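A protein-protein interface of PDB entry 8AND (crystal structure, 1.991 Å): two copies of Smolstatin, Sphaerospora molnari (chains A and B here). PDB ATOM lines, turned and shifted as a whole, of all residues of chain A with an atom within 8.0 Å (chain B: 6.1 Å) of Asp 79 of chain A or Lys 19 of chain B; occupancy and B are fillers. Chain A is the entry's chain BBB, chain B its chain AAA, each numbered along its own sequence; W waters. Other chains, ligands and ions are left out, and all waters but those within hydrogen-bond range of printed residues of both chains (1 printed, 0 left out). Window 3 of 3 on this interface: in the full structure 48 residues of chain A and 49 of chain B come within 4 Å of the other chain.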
ATOM      1  N   MET A  57      -1.187 -23.153 -31.369  1.00  0.00           N
ATOM      2  CA  MET A  57      -0.216 -22.827 -32.441  1.00  0.00           C
ATOM      3  C   MET A  57       0.328 -24.146 -33.005  1.00  0.00           C
ATOM      4  O   MET A  57       0.918 -24.930 -32.238  1.00  0.00           O
ATOM      5  CB  MET A  57       0.924 -21.944 -31.899  1.00  0.00           C
ATOM      6  CG  MET A  57       0.477 -20.744 -31.076  1.00  0.00           C
ATOM      7  SD  MET A  57      -0.441 -19.532 -32.013  1.00  0.00           S
ATOM      8  CE  MET A  57       0.020 -18.054 -31.119  1.00  0.00           C
ATOM      9  N   GLY A  75      -4.176  -7.299 -22.209  1.00  0.00           N
ATOM     10  CA  GLY A  75      -3.114  -6.328 -21.933  1.00  0.00           C
ATOM     11  C   GLY A  75      -1.743  -6.800 -22.382  1.00  0.00           C
ATOM     12  O   GLY A  75      -0.851  -5.948 -22.520  1.00  0.00           O
ATOM     13  N   SER A  76      -1.538  -8.109 -22.577  1.00  0.00           N
ATOM     14  CA  SER A  76      -0.260  -8.620 -23.113  1.00  0.00           C
ATOM     15  C   SER A  76      -0.375  -8.845 -24.623  1.00  0.00           C
ATOM     16  O   SER A  76      -1.457  -9.182 -25.132  1.00  0.00           O
ATOM     17  CB  SER A  76       0.185  -9.874 -22.367  1.00  0.00           C
ATOM     18  OG  SER A  76       0.500  -9.593 -20.996  1.00  0.00           O
ATOM     19  N   THR A  77       0.737  -8.679 -25.312  1.00  0.00           N
ATOM     20  CA  THR A  77       0.948  -9.120 -26.711  1.00  0.00           C
ATOM     21  C   THR A  77       2.337  -9.779 -26.801  1.00  0.00           C
ATOM     22  O   THR A  77       3.003  -9.956 -25.766  1.00  0.00           O
ATOM     23  CB  THR A  77       0.796  -7.934 -27.674  1.00  0.00           C
ATOM     24  OG1 THR A  77       1.977  -7.125 -27.585  1.00  0.00           O
ATOM     25  CG2 THR A  77      -0.446  -7.106 -27.395  1.00  0.00           C
ATOM     26  N   GLY A  78       2.749 -10.183 -27.981  1.00  0.00           N
ATOM     27  CA  GLY A  78       4.121 -10.672 -28.198  1.00  0.00           C
ATOM     28  C   GLY A  78       5.164  -9.605 -27.847  1.00  0.00           C
ATOM     29  O   GLY A  78       6.344  -9.991 -27.629  1.00  0.00           O
ATOM     30  N   ASP A  79       4.771  -8.324 -27.791  1.00  0.00           N
ATOM     31  CA  ASP A  79       5.661  -7.161 -27.537  1.00  0.00           C
ATOM     32  C   ASP A  79       5.388  -6.478 -26.190  1.00  0.00           C
ATOM     33  O   ASP A  79       6.309  -5.828 -25.677  1.00  0.00           O
ATOM     34  CB  ASP A  79       5.440  -6.067 -28.596  1.00  0.00           C
ATOM     35  CG  ASP A  79       6.270  -6.317 -29.819  1.00  0.00           C
ATOM     36  OD1 ASP A  79       7.069  -7.283 -29.786  1.00  0.00           O
ATOM     37  OD2 ASP A  79       6.088  -5.579 -30.790  1.00  0.00           O
ATOM     38  N   ILE A  80       4.167  -6.525 -25.682  1.00  0.00           N
ATOM     39  CA  ILE A  80       3.757  -5.764 -24.470  1.00  0.00           C
ATOM     40  C   ILE A  80       3.521  -6.754 -23.352  1.00  0.00           C
ATOM     41  O   ILE A  80       2.651  -7.651 -23.500  1.00  0.00           O
ATOM     42  CB  ILE A  80       2.519  -4.899 -24.740  1.00  0.00           C
ATOM     43  CG1 ILE A  80       2.797  -3.893 -25.858  1.00  0.00           C
ATOM     44  CG2 ILE A  80       2.040  -4.194 -23.485  1.00  0.00           C
ATOM     45  CD1 ILE A  80       1.567  -3.098 -26.255  1.00  0.00           C
ATOM     46  N   LYS A  81       4.249  -6.590 -22.253  1.00  0.00           N
ATOM     47  CA  LYS A  81       4.036  -7.391 -21.045  1.00  0.00           C
ATOM     48  C   LYS A  81       4.093  -8.864 -21.430  1.00  0.00           C
ATOM     49  O   LYS A  81       3.282  -9.686 -20.923  1.00  0.00           O
ATOM     50  CB  LYS A  81       2.698  -7.031 -20.392  1.00  0.00           C
ATOM     51  CG  LYS A  81       2.695  -5.677 -19.717  1.00  0.00           C
ATOM     52  CD  LYS A  81       1.577  -5.518 -18.722  1.00  0.00           C
ATOM     53  CE  LYS A  81       1.381  -4.071 -18.347  1.00  0.00           C
ATOM     54  NZ  LYS A  81       1.069  -3.265 -19.549  1.00  0.00           N
ATOM     55  N   SER A  82       5.022  -9.186 -22.306  1.00  0.00           N
ATOM     56  CA  SER A  82       5.098 -10.520 -22.944  1.00  0.00           C
ATOM     57  C   SER A  82       5.544 -11.562 -21.918  1.00  0.00           C
ATOM     58  O   SER A  82       5.325 -12.736 -22.173  1.00  0.00           O
ATOM     59  CB  SER A  82       5.998 -10.492 -24.118  1.00  0.00           C
ATOM     60  OG  SER A  82       7.183  -9.729 -23.806  1.00  0.00           O
ATOM     61  N   HIS A  83       6.062 -11.137 -20.771  1.00  0.00           N
ATOM     62  CA  HIS A  83       6.505 -12.037 -19.678  1.00  0.00           C
ATOM     63  C   HIS A  83       5.302 -12.741 -19.057  1.00  0.00           C
ATOM     64  O   HIS A  83       5.507 -13.800 -18.459  1.00  0.00           O
ATOM     65  CB  HIS A  83       7.286 -11.260 -18.612  1.00  0.00           C
ATOM     66  CG  HIS A  83       6.464 -10.315 -17.811  1.00  0.00           C
ATOM     67  ND1 HIS A  83       6.193  -9.028 -18.235  1.00  0.00           N
ATOM     68  CD2 HIS A  83       5.871 -10.456 -16.605  1.00  0.00           C
ATOM     69  CE1 HIS A  83       5.461  -8.422 -17.337  1.00  0.00           C
ATOM     70  NE2 HIS A  83       5.258  -9.279 -16.315  1.00  0.00           N
ATOM     71  N   ILE A  85       2.742 -13.968 -20.876  1.00  0.00           N
ATOM     72  CA  ILE A  85       2.219 -15.024 -21.773  1.00  0.00           C
ATOM     73  C   ILE A  85       2.628 -16.375 -21.179  1.00  0.00           C
ATOM     74  O   ILE A  85       3.765 -16.514 -20.761  1.00  0.00           O
ATOM     75  CB  ILE A  85       2.726 -14.851 -23.209  1.00  0.00           C
ATOM     76  CG1 ILE A  85       2.287 -13.501 -23.779  1.00  0.00           C
ATOM     77  CG2 ILE A  85       2.274 -16.024 -24.074  1.00  0.00           C
ATOM     78  CD1 ILE A  85       2.982 -13.113 -25.044  1.00  0.00           C
ATOM     79  N   ASP B  14      -0.403 -14.628 -38.789  1.00  0.00           N
ATOM     80  CA  ASP B  14      -0.467 -13.163 -39.006  1.00  0.00           C
ATOM     81  C   ASP B  14       0.633 -12.539 -38.158  1.00  0.00           C
ATOM     82  O   ASP B  14       1.287 -13.271 -37.390  1.00  0.00           O
ATOM     83  CB  ASP B  14      -1.874 -12.638 -38.715  1.00  0.00           C
ATOM     84  CG  ASP B  14      -2.405 -12.940 -37.326  1.00  0.00           C
ATOM     85  OD1 ASP B  14      -1.583 -13.174 -36.359  1.00  0.00           O
ATOM     86  OD2 ASP B  14      -3.639 -12.967 -37.199  1.00  0.00           O
ATOM     87  N   ALA B  15       0.851 -11.237 -38.293  1.00  0.00           N
ATOM     88  CA  ALA B  15       1.978 -10.558 -37.622  1.00  0.00           C
ATOM     89  C   ALA B  15       1.833 -10.739 -36.115  1.00  0.00           C
ATOM     90  O   ALA B  15       2.820 -11.019 -35.417  1.00  0.00           O
ATOM     91  CB  ALA B  15       2.034  -9.104 -38.003  1.00  0.00           C
ATOM     92  N   TYR B  16       0.622 -10.586 -35.620  1.00  0.00           N
ATOM     93  CA  TYR B  16       0.313 -10.615 -34.185  1.00  0.00           C
ATOM     94  C   TYR B  16       0.700 -11.978 -33.585  1.00  0.00           C
ATOM     95  O   TYR B  16       1.452 -12.035 -32.597  1.00  0.00           O
ATOM     96  CB  TYR B  16      -1.174 -10.316 -33.977  1.00  0.00           C
ATOM     97  CG  TYR B  16      -1.560 -10.205 -32.528  1.00  0.00           C
ATOM     98  CD1 TYR B  16      -1.429  -9.004 -31.846  1.00  0.00           C
ATOM     99  CD2 TYR B  16      -2.054 -11.292 -31.834  1.00  0.00           C
ATOM    100  CE1 TYR B  16      -1.793  -8.886 -30.517  1.00  0.00           C
ATOM    101  CE2 TYR B  16      -2.418 -11.192 -30.504  1.00  0.00           C
ATOM    102  CZ  TYR B  16      -2.298  -9.982 -29.843  1.00  0.00           C
ATOM    103  OH  TYR B  16      -2.617  -9.912 -28.517  1.00  0.00           O
ATOM    104  N   THR B  17       0.159 -13.060 -34.107  1.00  0.00           N
ATOM    105  CA  THR B  17       0.431 -14.416 -33.553  1.00  0.00           C
ATOM    106  C   THR B  17       1.878 -14.840 -33.807  1.00  0.00           C
ATOM    107  O   THR B  17       2.437 -15.556 -32.960  1.00  0.00           O
ATOM    108  CB  THR B  17      -0.551 -15.447 -34.087  1.00  0.00           C
ATOM    109  OG1 THR B  17      -0.568 -15.337 -35.510  1.00  0.00           O
ATOM    110  CG2 THR B  17      -1.925 -15.247 -33.499  1.00  0.00           C
ATOM    111  N   THR B  18       2.479 -14.423 -34.918  1.00  0.00           N
ATOM    112  CA  THR B  18       3.898 -14.772 -35.194  1.00  0.00           C
ATOM    113  C   THR B  18       4.800 -14.211 -34.083  1.00  0.00           C
ATOM    114  O   THR B  18       5.699 -14.920 -33.634  1.00  0.00           O
ATOM    115  CB  THR B  18       4.334 -14.269 -36.566  1.00  0.00           C
ATOM    116  OG1 THR B  18       3.564 -14.997 -37.519  1.00  0.00           O
ATOM    117  CG2 THR B  18       5.835 -14.417 -36.777  1.00  0.00           C
ATOM    118  N   LYS B  19       4.548 -12.989 -33.635  1.00  0.00           N
ATOM    119  CA  LYS B  19       5.323 -12.383 -32.538  1.00  0.00           C
ATOM    120  C   LYS B  19       5.142 -13.194 -31.262  1.00  0.00           C
ATOM    121  O   LYS B  19       6.107 -13.312 -30.484  1.00  0.00           O
ATOM    122  CB  LYS B  19       4.859 -10.962 -32.265  1.00  0.00           C
ATOM    123  CG  LYS B  19       5.436  -9.916 -33.171  1.00  0.00           C
ATOM    124  CD  LYS B  19       5.235  -8.537 -32.590  1.00  0.00           C
ATOM    125  CE  LYS B  19       5.576  -7.484 -33.616  1.00  0.00           C
ATOM    126  NZ  LYS B  19       5.476  -6.126 -33.045  1.00  0.00           N
ATOM    127  N   ILE B  20       3.940 -13.687 -31.017  1.00  0.00           N
ATOM    128  CA  ILE B  20       3.681 -14.512 -29.808  1.00  0.00           C
ATOM    129  C   ILE B  20       4.483 -15.820 -29.887  1.00  0.00           C
ATOM    130  O   ILE B  20       5.143 -16.196 -28.891  1.00  0.00           O
ATOM    131  CB  ILE B  20       2.168 -14.718 -29.634  1.00  0.00           C
ATOM    132  CG1 ILE B  20       1.523 -13.405 -29.184  1.00  0.00           C
ATOM    133  CG2 ILE B  20       1.850 -15.864 -28.667  1.00  0.00           C
ATOM    134  CD1 ILE B  20       0.007 -13.371 -29.334  1.00  0.00           C
ATOM    135  N   VAL B  21       4.496 -16.484 -31.019  1.00  0.00           N
ATOM    136  CA  VAL B  21       5.243 -17.771 -31.145  1.00  0.00           C
ATOM    137  C   VAL B  21       6.739 -17.486 -30.963  1.00  0.00           C
ATOM    138  O   VAL B  21       7.467 -18.282 -30.304  1.00  0.00           O
ATOM    139  CB  VAL B  21       4.953 -18.458 -32.483  1.00  0.00           C
ATOM    140  CG1 VAL B  21       5.831 -19.698 -32.632  1.00  0.00           C
ATOM    141  CG2 VAL B  21       3.470 -18.855 -32.561  1.00  0.00           C
ATOM    142  N   LYS B  22       7.219 -16.410 -31.561  1.00  0.00           N
ATOM    143  CA  LYS B  22       8.650 -16.049 -31.472  1.00  0.00           C
ATOM    144  C   LYS B  22       8.998 -15.764 -30.008  1.00  0.00           C
ATOM    145  O   LYS B  22      10.041 -16.210 -29.558  1.00  0.00           O
ATOM    146  CB  LYS B  22       8.967 -14.842 -32.351  1.00  0.00           C
ATOM    147  CG  LYS B  22      10.423 -14.411 -32.262  1.00  0.00           C
ATOM    148  CD  LYS B  22      10.869 -13.571 -33.413  1.00  0.00           C
ATOM    149  CE  LYS B  22      11.927 -12.565 -32.994  1.00  0.00           C
ATOM    150  NZ  LYS B  22      12.300 -11.660 -34.102  1.00  0.00           N
ATOM    151  N   ALA B  23       8.113 -15.083 -29.286  1.00  0.00           N
ATOM    152  CA  ALA B  23       8.359 -14.797 -27.858  1.00  0.00           C
ATOM    153  C   ALA B  23       8.477 -16.091 -27.058  1.00  0.00           C
ATOM    154  O   ALA B  23       9.210 -16.092 -26.039  1.00  0.00           O
ATOM    155  CB  ALA B  23       7.291 -13.922 -27.266  1.00  0.00           C
ATOM    156  N   MET B  24       7.801 -17.160 -27.472  1.00  0.00           N
ATOM    157  CA  MET B  24       7.774 -18.413 -26.673  1.00  0.00           C
ATOM    158  C   MET B  24       8.945 -19.336 -26.994  1.00  0.00           C
ATOM    159  O   MET B  24       9.025 -20.407 -26.353  1.00  0.00           O
ATOM    160  CB  MET B  24       6.464 -19.175 -26.910  1.00  0.00           C
ATOM    161  CG  MET B  24       5.260 -18.500 -26.314  1.00  0.00           C
ATOM    162  SD  MET B  24       5.353 -18.259 -24.549  1.00  0.00           S
ATOM    163  CE  MET B  24       6.204 -16.689 -24.425  1.00  0.00           C
HETATM  164  O   HOH W   1       1.795  -9.995 -30.637  1.00  0.00           O
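The side-chain amino group of Lys 19 of chain B lies within salt-bridge range of the side-chain carboxylate of Asp 79 of chain A, at 3.8 Å.
OG1 of Thr 77 of chain A lies close to N of Asp 79 of chain A (3.0 Å). O of Lys 81 of chain A sits at hydrogen-bond distance from OG of Ser 76 of chain A, at 2.8 Å. The side-chain hydroxyl of Thr 17 of chain B sits at hydrogen-bond distance from the side-chain carboxylate of Asp 14 of chain B (2.5 Å). N of Ile 80 of chain A is in hydrogen-bond range of OG1 of Thr 77 of chain A, 3.0 Å away. N of Tyr 16 of chain B lies close to OD1 of Asp 14 of chain B (3.5 Å).
Among the printed residues, merely in contact across the chains: Gly 78 of chain A with Ile 20 of chain B (3.7 Å), Ser 76 of chain A with Tyr 16 of chain B (3.7 Å), Thr 77 of chain A with Tyr 16 of chain B (3.7 Å), Met 57 of chain A with Ile 20 of chain B (3.8 Å), Met 57 of chain A with Val 21 of chain B (3.8 Å), Ile 85 of chain A with Met 24 of chain B (3.8 Å) and Met 57 of chain A with Thr 17 of chain B (3.9 Å).
Of the printed residues of chain B, Asp 79 of chain A touches Lys 19 (2.4 Å). Of the printed residues of chain A, Ile 20 of chain B touches Met 57 and Gly 78. Printed residues of chain B within 4 Å of Met 57 of chain A: Thr 17, Ile 20 and Val 21. Ser 82 of chain A touches none of the printed residues of chain B. His 83 of chain A touches none of the printed residues of chain B. The nearest printed residue of chain A that does not touch Lys 19 of chain B is Gly 78 of chain A (4.02 Å). The nearest printed residue of chain A that does not touch Thr 17 of chain B is Gly 78 of chain A (7.0 Å).
Hydrophobic or aromatic side chains of chain A within 4 Å of the printed part of chain B: Met 57 and Ile 85. Among the printed residues, Asp or Glu carboxylates within 4 Å of a Lys or Arg side-chain nitrogen of the other chain: Asp 79 of chain A with Lys 19 of chain B.
No position is printed for both chains. Of the 8 pairs that touch across the chains among the printed residues, none has its exchanged pair printed and touching as well.
Water W1 lies within hydrogen-bond range of N of Gly 78 of chain A (2.8 Å) and O of Tyr 16 of chain B (2.8 Å).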
